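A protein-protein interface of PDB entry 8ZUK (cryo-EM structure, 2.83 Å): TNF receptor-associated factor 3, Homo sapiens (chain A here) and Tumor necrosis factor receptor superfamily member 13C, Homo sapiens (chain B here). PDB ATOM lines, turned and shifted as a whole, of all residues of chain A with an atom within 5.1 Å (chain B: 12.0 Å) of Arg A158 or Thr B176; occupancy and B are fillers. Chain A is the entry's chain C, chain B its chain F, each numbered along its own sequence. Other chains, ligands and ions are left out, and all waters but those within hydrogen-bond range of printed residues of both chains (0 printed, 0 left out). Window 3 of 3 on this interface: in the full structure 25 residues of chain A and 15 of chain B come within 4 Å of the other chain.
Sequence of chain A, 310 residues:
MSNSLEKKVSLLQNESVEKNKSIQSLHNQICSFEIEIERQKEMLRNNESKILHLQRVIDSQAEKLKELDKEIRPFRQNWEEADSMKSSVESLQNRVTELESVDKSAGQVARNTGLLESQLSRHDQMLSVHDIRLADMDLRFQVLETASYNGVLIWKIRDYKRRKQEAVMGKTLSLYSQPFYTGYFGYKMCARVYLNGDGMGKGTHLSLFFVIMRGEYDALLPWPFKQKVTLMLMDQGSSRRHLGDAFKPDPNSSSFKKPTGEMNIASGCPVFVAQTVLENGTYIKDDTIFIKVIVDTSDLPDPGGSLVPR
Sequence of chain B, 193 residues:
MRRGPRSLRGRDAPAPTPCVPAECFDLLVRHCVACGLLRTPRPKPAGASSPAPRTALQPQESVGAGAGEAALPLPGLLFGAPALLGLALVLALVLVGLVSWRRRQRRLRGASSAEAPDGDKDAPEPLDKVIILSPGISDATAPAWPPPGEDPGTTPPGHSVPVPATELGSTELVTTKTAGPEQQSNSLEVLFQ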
ATOM      1  N   GLN A 142      -4.670 -21.120 -29.736  1.00  0.00           N
ATOM      2  CA  GLN A 142      -4.335 -22.409 -29.142  1.00  0.00           C
ATOM      3  C   GLN A 142      -5.574 -23.124 -28.620  1.00  0.00           C
ATOM      4  O   GLN A 142      -5.690 -24.348 -28.746  1.00  0.00           O
ATOM      5  CB  GLN A 142      -3.314 -22.216 -28.021  1.00  0.00           C
ATOM      6  CG  GLN A 142      -2.768 -23.513 -27.459  1.00  0.00           C
ATOM      7  CD  GLN A 142      -1.982 -24.307 -28.484  1.00  0.00           C
ATOM      8  OE1 GLN A 142      -2.463 -25.309 -29.012  1.00  0.00           O
ATOM      9  NE2 GLN A 142      -0.764 -23.861 -28.772  1.00  0.00           N
ATOM     10  N   THR A 146      -6.780 -26.856 -30.111  1.00  0.00           N
ATOM     11  CA  THR A 146      -6.925 -28.059 -29.304  1.00  0.00           C
ATOM     12  C   THR A 146      -8.363 -28.309 -28.867  1.00  0.00           C
ATOM     13  O   THR A 146      -8.604 -29.202 -28.050  1.00  0.00           O
ATOM     14  CB  THR A 146      -6.018 -27.980 -28.075  1.00  0.00           C
ATOM     15  OG1 THR A 146      -6.422 -26.878 -27.256  1.00  0.00           O
ATOM     16  CG2 THR A 146      -4.571 -27.790 -28.494  1.00  0.00           C
ATOM     17  N   LYS A 156      -2.437 -32.575 -22.714  1.00  0.00           N
ATOM     18  CA  LYS A 156      -0.989 -32.723 -22.721  1.00  0.00           C
ATOM     19  C   LYS A 156      -0.377 -31.624 -21.864  1.00  0.00           C
ATOM     20  O   LYS A 156      -0.584 -30.435 -22.132  1.00  0.00           O
ATOM     21  CB  LYS A 156      -0.447 -32.662 -24.149  1.00  0.00           C
ATOM     22  CG  LYS A 156       1.057 -32.837 -24.253  1.00  0.00           C
ATOM     23  CD  LYS A 156       1.494 -32.958 -25.703  1.00  0.00           C
ATOM     24  CE  LYS A 156       3.007 -32.992 -25.822  1.00  0.00           C
ATOM     25  NZ  LYS A 156       3.464 -32.563 -27.172  1.00  0.00           N
ATOM     26  N   ILE A 157       0.375 -32.017 -20.841  1.00  0.00           N
ATOM     27  CA  ILE A 157       1.013 -31.084 -19.919  1.00  0.00           C
ATOM     28  C   ILE A 157       2.517 -31.304 -20.034  1.00  0.00           C
ATOM     29  O   ILE A 157       3.060 -32.259 -19.467  1.00  0.00           O
ATOM     30  CB  ILE A 157       0.532 -31.268 -18.476  1.00  0.00           C
ATOM     31  CG1 ILE A 157      -0.985 -31.094 -18.394  1.00  0.00           C
ATOM     32  CG2 ILE A 157       1.230 -30.281 -17.554  1.00  0.00           C
ATOM     33  CD1 ILE A 157      -1.558 -31.379 -17.025  1.00  0.00           C
ATOM     34  N   ARG A 158       3.190 -30.423 -20.767  1.00  0.00           N
ATOM     35  CA  ARG A 158       4.631 -30.498 -20.934  1.00  0.00           C
ATOM     36  C   ARG A 158       5.337 -29.806 -19.771  1.00  0.00           C
ATOM     37  O   ARG A 158       4.733 -29.060 -18.998  1.00  0.00           O
ATOM     38  CB  ARG A 158       5.046 -29.871 -22.264  1.00  0.00           C
ATOM     39  CG  ARG A 158       4.321 -30.448 -23.469  1.00  0.00           C
ATOM     40  CD  ARG A 158       4.409 -29.525 -24.675  1.00  0.00           C
ATOM     41  NE  ARG A 158       5.743 -29.510 -25.263  1.00  0.00           N
ATOM     42  CZ  ARG A 158       6.638 -28.553 -25.066  1.00  0.00           C
ATOM     43  NH1 ARG A 158       6.377 -27.509 -24.298  1.00  0.00           N
ATOM     44  NH2 ARG A 158       7.828 -28.645 -25.655  1.00  0.00           N
ATOM     45  N   ASP A 159       6.640 -30.069 -19.653  1.00  0.00           N
ATOM     46  CA  ASP A 159       7.482 -29.489 -18.605  1.00  0.00           C
ATOM     47  C   ASP A 159       6.909 -29.783 -17.217  1.00  0.00           C
ATOM     48  O   ASP A 159       6.668 -28.887 -16.405  1.00  0.00           O
ATOM     49  CB  ASP A 159       7.663 -27.983 -18.824  1.00  0.00           C
ATOM     50  CG  ASP A 159       8.196 -27.655 -20.205  1.00  0.00           C
ATOM     51  OD1 ASP A 159       8.863 -28.522 -20.808  1.00  0.00           O
ATOM     52  OD2 ASP A 159       7.947 -26.529 -20.687  1.00  0.00           O
ATOM     53  N   TYR A 160       6.693 -31.075 -16.959  1.00  0.00           N
ATOM     54  CA  TYR A 160       6.103 -31.492 -15.693  1.00  0.00           C
ATOM     55  C   TYR A 160       7.030 -31.222 -14.514  1.00  0.00           C
ATOM     56  O   TYR A 160       6.554 -30.925 -13.412  1.00  0.00           O
ATOM     57  CB  TYR A 160       5.735 -32.975 -15.751  1.00  0.00           C
ATOM     58  CG  TYR A 160       5.410 -33.583 -14.406  1.00  0.00           C
ATOM     59  CD1 TYR A 160       4.198 -33.326 -13.781  1.00  0.00           C
ATOM     60  CD2 TYR A 160       6.314 -34.419 -13.763  1.00  0.00           C
ATOM     61  CE1 TYR A 160       3.896 -33.880 -12.551  1.00  0.00           C
ATOM     62  CE2 TYR A 160       6.021 -34.978 -12.536  1.00  0.00           C
ATOM     63  CZ  TYR A 160       4.812 -34.704 -11.934  1.00  0.00           C
ATOM     64  OH  TYR A 160       4.515 -35.259 -10.708  1.00  0.00           O
ATOM     65  N   ARG A 163       6.866 -27.484 -13.322  1.00  0.00           N
ATOM     66  CA  ARG A 163       5.544 -27.125 -12.820  1.00  0.00           C
ATOM     67  C   ARG A 163       5.199 -27.866 -11.536  1.00  0.00           C
ATOM     68  O   ARG A 163       4.486 -27.319 -10.687  1.00  0.00           O
ATOM     69  CB  ARG A 163       4.488 -27.390 -13.895  1.00  0.00           C
ATOM     70  CG  ARG A 163       4.552 -26.398 -15.045  1.00  0.00           C
ATOM     71  CD  ARG A 163       3.370 -26.536 -15.988  1.00  0.00           C
ATOM     72  NE  ARG A 163       3.590 -25.787 -17.220  1.00  0.00           N
ATOM     73  CZ  ARG A 163       3.467 -26.296 -18.438  1.00  0.00           C
ATOM     74  NH1 ARG A 163       3.096 -27.550 -18.629  1.00  0.00           N
ATOM     75  NH2 ARG A 163       3.720 -25.523 -19.492  1.00  0.00           N
ATOM     76  N   ASP A 287       9.278 -35.396 -19.870  1.00  0.00           N
ATOM     77  CA  ASP A 287       8.718 -34.466 -18.893  1.00  0.00           C
ATOM     78  C   ASP A 287       7.309 -34.034 -19.283  1.00  0.00           C
ATOM     79  O   ASP A 287       6.965 -32.852 -19.179  1.00  0.00           O
ATOM     80  CB  ASP A 287       9.628 -33.246 -18.734  1.00  0.00           C
ATOM     81  CG  ASP A 287       9.547 -32.640 -17.348  1.00  0.00           C
ATOM     82  OD1 ASP A 287       9.294 -33.388 -16.383  1.00  0.00           O
ATOM     83  OD2 ASP A 287       9.739 -31.412 -17.224  1.00  0.00           O
ATOM     84  N   THR A 288       6.490 -34.982 -19.734  1.00  0.00           N
ATOM     85  CA  THR A 288       5.143 -34.688 -20.195  1.00  0.00           C
ATOM     86  C   THR A 288       4.193 -35.781 -19.728  1.00  0.00           C
ATOM     87  O   THR A 288       4.530 -36.967 -19.773  1.00  0.00           O
ATOM     88  CB  THR A 288       5.095 -34.569 -21.726  1.00  0.00           C
ATOM     89  OG1 THR A 288       6.041 -33.583 -22.157  1.00  0.00           O
ATOM     90  CG2 THR A 288       3.709 -34.160 -22.191  1.00  0.00           C
ATOM     91  N   GLU B 172      -3.417 -21.219 -13.436  1.00  0.00           N
ATOM     92  CA  GLU B 172      -2.919 -20.841 -14.754  1.00  0.00           C
ATOM     93  C   GLU B 172      -3.323 -21.914 -15.750  1.00  0.00           C
ATOM     94  O   GLU B 172      -2.915 -23.071 -15.614  1.00  0.00           O
ATOM     95  CB  GLU B 172      -1.396 -20.663 -14.749  1.00  0.00           C
ATOM     96  CG  GLU B 172      -0.840 -19.977 -13.512  1.00  0.00           C
ATOM     97  CD  GLU B 172      -1.084 -18.482 -13.513  1.00  0.00           C
ATOM     98  OE1 GLU B 172      -1.310 -17.917 -14.604  1.00  0.00           O
ATOM     99  OE2 GLU B 172      -1.050 -17.871 -12.425  1.00  0.00           O
ATOM    100  N   LEU B 173      -4.124 -21.531 -16.742  1.00  0.00           N
ATOM    101  CA  LEU B 173      -4.499 -22.466 -17.795  1.00  0.00           C
ATOM    102  C   LEU B 173      -3.281 -22.812 -18.640  1.00  0.00           C
ATOM    103  O   LEU B 173      -2.548 -21.925 -19.086  1.00  0.00           O
ATOM    104  CB  LEU B 173      -5.601 -21.861 -18.667  1.00  0.00           C
ATOM    105  CG  LEU B 173      -6.269 -22.769 -19.703  1.00  0.00           C
ATOM    106  CD1 LEU B 173      -7.753 -22.459 -19.798  1.00  0.00           C
ATOM    107  CD2 LEU B 173      -5.612 -22.621 -21.069  1.00  0.00           C
ATOM    108  N   VAL B 174      -3.063 -24.106 -18.856  1.00  0.00           N
ATOM    109  CA  VAL B 174      -1.929 -24.588 -19.635  1.00  0.00           C
ATOM    110  C   VAL B 174      -2.442 -25.521 -20.727  1.00  0.00           C
ATOM    111  O   VAL B 174      -3.210 -26.451 -20.452  1.00  0.00           O
ATOM    112  CB  VAL B 174      -0.867 -25.277 -18.755  1.00  0.00           C
ATOM    113  CG1 VAL B 174      -1.405 -26.547 -18.106  1.00  0.00           C
ATOM    114  CG2 VAL B 174       0.371 -25.582 -19.579  1.00  0.00           C
ATOM    115  N   THR B 175      -2.056 -25.234 -21.969  1.00  0.00           N
ATOM    116  CA  THR B 175      -2.381 -26.095 -23.106  1.00  0.00           C
ATOM    117  C   THR B 175      -1.448 -25.708 -24.244  1.00  0.00           C
ATOM    118  O   THR B 175      -1.455 -24.553 -24.679  1.00  0.00           O
ATOM    119  CB  THR B 175      -3.842 -25.946 -23.519  1.00  0.00           C
ATOM    120  OG1 THR B 175      -4.689 -26.464 -22.486  1.00  0.00           O
ATOM    121  CG2 THR B 175      -4.105 -26.708 -24.806  1.00  0.00           C
ATOM    122  N   THR B 176      -0.648 -26.659 -24.714  1.00  0.00           N
ATOM    123  CA  THR B 176       0.270 -26.408 -25.819  1.00  0.00           C
ATOM    124  C   THR B 176       0.737 -27.715 -26.445  1.00  0.00           C
ATOM    125  O   THR B 176      -0.072 -28.509 -26.920  1.00  0.00           O
ATOM    126  CB  THR B 176       1.498 -25.595 -25.363  1.00  0.00           C
ATOM    127  OG1 THR B 176       2.428 -25.480 -26.448  1.00  0.00           O
ATOM    128  CG2 THR B 176       2.178 -26.270 -24.183  1.00  0.00           C
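OG1 of Thr A146 is in hydrogen-bond range of O of Gln A142.
Of the printed residues of chain B, Gln A142 touches Thr B175 (3.2 Å).
Printed residues of chain B within 4 Å of Thr A146: Thr B175.
No residue of chain B comes within 4 Å of Lys A156.
No residue of chain B comes within 4 Å of Ile A157.
Printed residues of chain B within 4 Å of Arg A163: Val B174 (3.4 Å).
No residue of chain B comes within 4 Å of Thr A288.
Glu B172 touches none of the printed residues of chain A.
Leu B173 touches none of the printed residues of chain A.
Of the printed residues of chain A, Val B174 touches Arg A163 (3.4 Å).
Of the printed residues of chain A, Thr B175 touches Gln A142 (3.2 Å) and Thr A146 (3.4 Å).
Thr B176 touches just one residue of chain A: Arg A158 (3.98 Å).
CG of Gln A142 touches O of Thr B175, 3.2 Å away.
Thr A146 touches Thr B175 (OG1 to CG2, 3.4 Å).
Arg A158 touches Thr B176.
Val B174 touches Arg A163.
Of the 10 printed residues of chain A, 4 touch a printed residue of chain B.
Of the 5 printed residues of chain B, 3 touch a printed residue of chain A.
Along chain B the printed residues that touch a printed residue of chain A span positions 174 to 176.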
